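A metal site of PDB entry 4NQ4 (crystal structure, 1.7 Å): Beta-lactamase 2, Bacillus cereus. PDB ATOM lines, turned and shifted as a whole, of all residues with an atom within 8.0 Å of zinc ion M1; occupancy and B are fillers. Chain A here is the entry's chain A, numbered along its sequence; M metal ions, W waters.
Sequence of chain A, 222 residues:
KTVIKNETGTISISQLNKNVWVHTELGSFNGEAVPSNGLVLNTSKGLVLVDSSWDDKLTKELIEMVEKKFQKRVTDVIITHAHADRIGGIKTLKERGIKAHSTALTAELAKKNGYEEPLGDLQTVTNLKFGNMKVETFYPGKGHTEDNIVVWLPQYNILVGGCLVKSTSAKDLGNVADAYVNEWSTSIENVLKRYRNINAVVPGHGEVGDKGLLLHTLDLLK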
ATOM      1  N   VAL A  34      20.159  -8.213 -14.786  1.00  0.00           N
ATOM      2  CA  VAL A  34      20.372  -8.423 -16.195  1.00  0.00           C
ATOM      3  C   VAL A  34      19.211  -9.234 -16.746  1.00  0.00           C
ATOM      4  O   VAL A  34      19.024 -10.380 -16.320  1.00  0.00           O
ATOM      5  CB  VAL A  34      21.666  -9.160 -16.480  1.00  0.00           C
ATOM      6  CG1 VAL A  34      22.037  -8.985 -17.942  1.00  0.00           C
ATOM      7  CG2 VAL A  34      22.772  -8.683 -15.541  1.00  0.00           C
ATOM      8  N   PRO A  35      18.402  -8.608 -17.605  1.00  0.00           N
ATOM      9  CA  PRO A  35      17.233  -9.238 -18.210  1.00  0.00           C
ATOM     10  C   PRO A  35      17.602 -10.119 -19.413  1.00  0.00           C
ATOM     11  O   PRO A  35      18.572  -9.839 -20.092  1.00  0.00           O
ATOM     12  CB  PRO A  35      16.388  -8.057 -18.718  1.00  0.00           C
ATOM     13  CG  PRO A  35      17.415  -7.054 -19.030  1.00  0.00           C
ATOM     14  CD  PRO A  35      18.457  -7.184 -17.965  1.00  0.00           C
ATOM     15  N   SER A  36      16.848 -11.203 -19.581  1.00  0.00           N
ATOM     16  CA  SER A  36      17.058 -12.154 -20.676  1.00  0.00           C
ATOM     17  C   SER A  36      15.714 -12.516 -21.299  1.00  0.00           C
ATOM     18  O   SER A  36      14.708 -12.725 -20.576  1.00  0.00           O
ATOM     19  CB  SER A  36      17.771 -13.353 -20.120  1.00  0.00           C
ATOM     20  OG  SER A  36      17.820 -14.435 -21.022  1.00  0.00           O
ATOM     21  N   ASN A  37      15.666 -12.601 -22.629  1.00  0.00           N
ATOM     22  CA  ASN A  37      14.440 -12.938 -23.354  1.00  0.00           C
ATOM     23  C   ASN A  37      14.438 -14.331 -23.976  1.00  0.00           C
ATOM     24  O   ASN A  37      15.473 -14.769 -24.514  1.00  0.00           O
ATOM     25  CB  ASN A  37      14.190 -11.996 -24.539  1.00  0.00           C
ATOM     26  CG  ASN A  37      14.158 -10.548 -24.176  1.00  0.00           C
ATOM     27  OD1 ASN A  37      13.591 -10.107 -23.132  1.00  0.00           O
ATOM     28  ND2 ASN A  37      14.746  -9.757 -25.069  1.00  0.00           N
ATOM     29  N   ASP A  51      13.992 -21.180 -25.355  1.00  0.00           N
ATOM     30  CA  ASP A  51      14.954 -20.917 -24.290  1.00  0.00           C
ATOM     31  C   ASP A  51      14.284 -20.978 -22.900  1.00  0.00           C
ATOM     32  O   ASP A  51      13.097 -20.714 -22.740  1.00  0.00           O
ATOM     33  CB  ASP A  51      15.813 -19.640 -24.492  1.00  0.00           C
ATOM     34  CG  ASP A  51      16.914 -19.889 -25.519  1.00  0.00           C
ATOM     35  OD1 ASP A  51      17.042 -19.006 -26.401  1.00  0.00           O
ATOM     36  OD2 ASP A  51      17.590 -20.939 -25.460  1.00  0.00           O
ATOM     37  N   TRP A  54      18.010 -17.975 -16.728  1.00  0.00           N
ATOM     38  CA  TRP A  54      19.231 -17.939 -15.928  1.00  0.00           C
ATOM     39  C   TRP A  54      19.546 -19.100 -14.980  1.00  0.00           C
ATOM     40  O   TRP A  54      20.707 -19.473 -14.822  1.00  0.00           O
ATOM     41  CB  TRP A  54      19.255 -16.614 -15.138  1.00  0.00           C
ATOM     42  CG  TRP A  54      19.273 -15.400 -15.948  1.00  0.00           C
ATOM     43  CD1 TRP A  54      18.239 -14.541 -16.192  1.00  0.00           C
ATOM     44  CD2 TRP A  54      20.416 -14.847 -16.561  1.00  0.00           C
ATOM     45  NE1 TRP A  54      18.659 -13.476 -16.975  1.00  0.00           N
ATOM     46  CE2 TRP A  54      20.010 -13.639 -17.209  1.00  0.00           C
ATOM     47  CE3 TRP A  54      21.758 -15.259 -16.669  1.00  0.00           C
ATOM     48  CZ2 TRP A  54      20.883 -12.868 -17.969  1.00  0.00           C
ATOM     49  CZ3 TRP A  54      22.649 -14.465 -17.398  1.00  0.00           C
ATOM     50  CH2 TRP A  54      22.194 -13.261 -18.028  1.00  0.00           C
ATOM     51  N   THR A  80      18.967 -22.308 -27.515  1.00  0.00           N
ATOM     52  CA  THR A  80      19.595 -21.635 -28.637  1.00  0.00           C
ATOM     53  C   THR A  80      21.121 -21.386 -28.542  1.00  0.00           C
ATOM     54  O   THR A  80      21.768 -21.172 -29.557  1.00  0.00           O
ATOM     55  CB  THR A  80      18.913 -20.298 -28.994  1.00  0.00           C
ATOM     56  OG1 THR A  80      19.042 -19.375 -27.912  1.00  0.00           O
ATOM     57  CG2 THR A  80      17.432 -20.589 -29.386  1.00  0.00           C
ATOM     58  N   HIS A  81      21.646 -21.608 -27.357  1.00  0.00           N
ATOM     59  CA  HIS A  81      23.097 -21.832 -27.098  1.00  0.00           C
ATOM     60  C   HIS A  81      23.347 -22.215 -25.608  1.00  0.00           C
ATOM     61  O   HIS A  81      22.475 -22.083 -24.784  1.00  0.00           O
ATOM     62  CB  HIS A  81      24.050 -20.693 -27.573  1.00  0.00           C
ATOM     63  CG  HIS A  81      23.929 -19.417 -26.819  1.00  0.00           C
ATOM     64  ND1 HIS A  81      22.966 -18.481 -27.078  1.00  0.00           N
ATOM     65  CD2 HIS A  81      24.654 -18.922 -25.784  1.00  0.00           C
ATOM     66  CE1 HIS A  81      23.104 -17.465 -26.259  1.00  0.00           C
ATOM     67  NE2 HIS A  81      24.131 -17.697 -25.465  1.00  0.00           N
ATOM     68  N   HIS A  83      24.981 -20.908 -22.830  1.00  0.00           N
ATOM     69  CA  HIS A  83      25.229 -19.973 -21.747  1.00  0.00           C
ATOM     70  C   HIS A  83      24.051 -20.053 -20.757  1.00  0.00           C
ATOM     71  O   HIS A  83      22.933 -20.437 -21.150  1.00  0.00           O
ATOM     72  CB  HIS A  83      25.302 -18.499 -22.273  1.00  0.00           C
ATOM     73  CG  HIS A  83      26.602 -18.180 -22.940  1.00  0.00           C
ATOM     74  ND1 HIS A  83      26.764 -17.094 -23.789  1.00  0.00           N
ATOM     75  CD2 HIS A  83      27.822 -18.746 -22.827  1.00  0.00           C
ATOM     76  CE1 HIS A  83      28.023 -17.014 -24.157  1.00  0.00           C
ATOM     77  NE2 HIS A  83      28.693 -17.984 -23.573  1.00  0.00           N
ATOM     78  N   ALA A  84      24.296 -19.639 -19.507  1.00  0.00           N
ATOM     79  CA  ALA A  84      23.319 -19.846 -18.442  1.00  0.00           C
ATOM     80  C   ALA A  84      21.965 -19.192 -18.682  1.00  0.00           C
ATOM     81  O   ALA A  84      21.025 -19.631 -18.094  1.00  0.00           O
ATOM     82  CB  ALA A  84      23.859 -19.380 -17.096  1.00  0.00           C
ATOM     83  N   ASP A  85      21.895 -18.098 -19.436  1.00  0.00           N
ATOM     84  CA  ASP A  85      20.627 -17.421 -19.667  1.00  0.00           C
ATOM     85  C   ASP A  85      19.653 -18.157 -20.577  1.00  0.00           C
ATOM     86  O   ASP A  85      18.446 -17.893 -20.598  1.00  0.00           O
ATOM     87  CB  ASP A  85      20.866 -16.033 -20.230  1.00  0.00           C
ATOM     88  CG  ASP A  85      21.568 -16.016 -21.573  1.00  0.00           C
ATOM     89  OD1 ASP A  85      22.657 -16.603 -21.708  1.00  0.00           O
ATOM     90  OD2 ASP A  85      21.049 -15.247 -22.418  1.00  0.00           O
ATOM     91  N   ARG A  86      20.204 -19.100 -21.335  1.00  0.00           N
ATOM     92  CA  ARG A  86      19.466 -19.948 -22.265  1.00  0.00           C
ATOM     93  C   ARG A  86      19.214 -21.281 -21.616  1.00  0.00           C
ATOM     94  O   ARG A  86      18.112 -21.801 -21.741  1.00  0.00           O
ATOM     95  CB  ARG A  86      20.322 -20.276 -23.505  1.00  0.00           C
ATOM     96  CG  ARG A  86      20.903 -19.090 -24.302  1.00  0.00           C
ATOM     97  CD  ARG A  86      19.819 -18.172 -24.867  1.00  0.00           C
ATOM     98  NE  ARG A  86      19.596 -16.922 -24.159  1.00  0.00           N
ATOM     99  CZ  ARG A  86      18.528 -16.128 -24.340  1.00  0.00           C
ATOM    100  NH1 ARG A  86      18.425 -15.004 -23.674  1.00  0.00           N
ATOM    101  NH2 ARG A  86      17.555 -16.435 -25.166  1.00  0.00           N
ATOM    102  N   HIS A 144      27.984 -14.774 -31.702  1.00  0.00           N
ATOM    103  CA  HIS A 144      27.995 -14.569 -30.244  1.00  0.00           C
ATOM    104  C   HIS A 144      28.639 -15.731 -29.479  1.00  0.00           C
ATOM    105  O   HIS A 144      29.430 -15.511 -28.587  1.00  0.00           O
ATOM    106  CB  HIS A 144      26.546 -14.316 -29.753  1.00  0.00           C
ATOM    107  CG  HIS A 144      26.360 -14.452 -28.277  1.00  0.00           C
ATOM    108  ND1 HIS A 144      26.809 -13.512 -27.381  1.00  0.00           N
ATOM    109  CD2 HIS A 144      25.828 -15.457 -27.532  1.00  0.00           C
ATOM    110  CE1 HIS A 144      26.515 -13.899 -26.152  1.00  0.00           C
ATOM    111  NE2 HIS A 144      25.912 -15.060 -26.224  1.00  0.00           N
ATOM    112  N   THR A 145      28.251 -16.959 -29.863  1.00  0.00           N
ATOM    113  CA  THR A 145      28.989 -18.163 -29.545  1.00  0.00           C
ATOM    114  C   THR A 145      29.187 -19.057 -30.764  1.00  0.00           C
ATOM    115  O   THR A 145      28.654 -18.837 -31.891  1.00  0.00           O
ATOM    116  CB  THR A 145      28.194 -18.964 -28.537  1.00  0.00           C
ATOM    117  OG1 THR A 145      26.937 -19.291 -29.090  1.00  0.00           O
ATOM    118  CG2 THR A 145      28.079 -18.159 -27.207  1.00  0.00           C
ATOM    119  N   GLY A 162      17.949 -14.426 -30.625  1.00  0.00           N
ATOM    120  CA  GLY A 162      18.774 -14.835 -29.522  1.00  0.00           C
ATOM    121  C   GLY A 162      19.958 -13.893 -29.338  1.00  0.00           C
ATOM    122  O   GLY A 162      19.916 -12.778 -29.767  1.00  0.00           O
ATOM    123  N   CYS A 163      21.019 -14.399 -28.732  1.00  0.00           N
ATOM    124  CA  CYS A 163      22.120 -13.534 -28.288  1.00  0.00           C
ATOM    125  C   CYS A 163      23.105 -13.192 -29.453  1.00  0.00           C
ATOM    126  O   CYS A 163      24.011 -12.399 -29.286  1.00  0.00           O
ATOM    127  CB  CYS A 163      22.726 -14.161 -27.055  1.00  0.00           C
ATOM    128  SG  CYS A 163      21.396 -14.474 -25.864  1.00  0.00           S
ATOM    129  N   LEU A 164      22.910 -13.846 -30.588  1.00  0.00           N
ATOM    130  CA  LEU A 164      23.470 -13.478 -31.920  1.00  0.00           C
ATOM    131  C   LEU A 164      23.018 -12.071 -32.298  1.00  0.00           C
ATOM    132  O   LEU A 164      23.810 -11.344 -32.962  1.00  0.00           O
ATOM    133  CB  LEU A 164      23.064 -14.462 -33.013  1.00  0.00           C
ATOM    134  CG  LEU A 164      23.632 -14.300 -34.414  1.00  0.00           C
ATOM    135  CD1 LEU A 164      25.108 -14.749 -34.466  1.00  0.00           C
ATOM    136  CD2 LEU A 164      22.721 -15.163 -35.260  1.00  0.00           C
ATOM    137  N   VAL A 165      21.841 -11.629 -31.803  1.00  0.00           N
ATOM    138  CA  VAL A 165      21.265 -10.359 -32.305  1.00  0.00           C
ATOM    139  C   VAL A 165      21.204  -9.378 -31.125  1.00  0.00           C
ATOM    140  O   VAL A 165      20.632  -9.656 -30.081  1.00  0.00           O
ATOM    141  CB  VAL A 165      19.915 -10.554 -33.067  1.00  0.00           C
ATOM    142  CG1 VAL A 165      19.393  -9.117 -33.486  1.00  0.00           C
ATOM    143  CG2 VAL A 165      20.103 -11.472 -34.275  1.00  0.00           C
ATOM    144  N   LYS A 166      21.845  -8.211 -31.309  1.00  0.00           N
ATOM    145  CA  LYS A 166      21.916  -7.168 -30.280  1.00  0.00           C
ATOM    146  C   LYS A 166      20.729  -6.235 -30.465  1.00  0.00           C
ATOM    147  O   LYS A 166      20.327  -5.928 -31.618  1.00  0.00           O
ATOM    148  CB  LYS A 166      23.233  -6.369 -30.413  1.00  0.00           C
ATOM    149  CG  LYS A 166      24.532  -7.178 -30.413  1.00  0.00           C
ATOM    150  CD  LYS A 166      24.521  -8.204 -29.270  1.00  0.00           C
ATOM    151  CE  LYS A 166      24.694  -7.636 -27.870  1.00  0.00           C
ATOM    152  NZ  LYS A 166      25.491  -8.563 -27.033  1.00  0.00           N
ATOM    153  N   PRO A 203      15.635  -9.989 -29.844  1.00  0.00           N
ATOM    154  CA  PRO A 203      17.034 -10.222 -29.423  1.00  0.00           C
ATOM    155  C   PRO A 203      17.093 -10.983 -28.113  1.00  0.00           C
ATOM    156  O   PRO A 203      16.029 -11.093 -27.435  1.00  0.00           O
ATOM    157  CB  PRO A 203      17.586  -8.784 -29.225  1.00  0.00           C
ATOM    158  CG  PRO A 203      16.411  -8.095 -28.688  1.00  0.00           C
ATOM    159  CD  PRO A 203      15.201  -8.639 -29.440  1.00  0.00           C
ATOM    160  N   GLY A 204      18.251 -11.536 -27.764  1.00  0.00           N
ATOM    161  CA  GLY A 204      18.363 -12.315 -26.531  1.00  0.00           C
ATOM    162  C   GLY A 204      18.220 -11.448 -25.277  1.00  0.00           C
ATOM    163  O   GLY A 204      17.928 -11.926 -24.184  1.00  0.00           O
ATOM    164  N   HIS A 205      18.544 -10.154 -25.432  1.00  0.00           N
ATOM    165  CA  HIS A 205      18.475  -9.188 -24.365  1.00  0.00           C
ATOM    166  C   HIS A 205      18.061  -7.856 -24.972  1.00  0.00           C
ATOM    167  O   HIS A 205      18.677  -7.396 -25.945  1.00  0.00           O
ATOM    168  CB  HIS A 205      19.835  -8.999 -23.714  1.00  0.00           C
ATOM    169  CG  HIS A 205      20.508 -10.287 -23.370  1.00  0.00           C
ATOM    170  ND1 HIS A 205      20.321 -10.921 -22.162  1.00  0.00           N
ATOM    171  CD2 HIS A 205      21.369 -11.049 -24.066  1.00  0.00           C
ATOM    172  CE1 HIS A 205      20.997 -12.059 -22.163  1.00  0.00           C
ATOM    173  NE2 HIS A 205      21.691 -12.119 -23.281  1.00  0.00           N
HETATM  174 ZN    ZN M   1      22.298 -14.049 -23.755  1.00  0.00          ZN
HETATM  175 ZN    ZN M   2      25.277 -16.127 -24.612  1.00  0.00          ZN
HETATM  176  O   HOH W   1      24.441 -14.360 -23.430  1.00  0.00           O
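Residues that only touch zinc ion M1: Arg 86. Of the 22 residues printed, 4 come within 4 Å of zinc ion M1. Along chain A the residues within 4 Å of zinc ion M1 span positions 85 to 205.
The side-chain carboxylate (OD1) of Asp 51 is in salt-bridge range of the guanidinium group (NH2) of Arg 86, at 2.9 Å. NH1 of Arg 86 sits at hydrogen-bond distance from OG of Ser 36 (2.8 Å). The guanidinium group (NH2) of Arg 86 lies within hydrogen-bond range of the backbone carbonyl oxygen (O) of Asn 37. The side-chain carboxylate (OD1) of Asp 85 lies within salt-bridge range of the guanidinium group (NE) of Arg 86, 3.9 Å away. A ring nitrogen (ND1) of His 205 is in hydrogen-bond range of the backbone carbonyl oxygen of Pro 35, at 2.9 Å. O of Gly 204 is in hydrogen-bond range of NH1 of Arg 86, at 3.2 Å. The side-chain sulfur (SG) of Cys 163 lies close to the guanidinium group (NE) of Arg 86 (3.5 Å).
Zinc ion M1 is bound by a ring nitrogen (NE2) of His 205 (2.1 Å), the side-chain carboxylate of Asp 85 (2.2 Å), water W1 (2.2 Å) and the side-chain sulfur of Cys 163 (2.3 Å). Zinc ion M1 has four donor atoms within binding distance.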
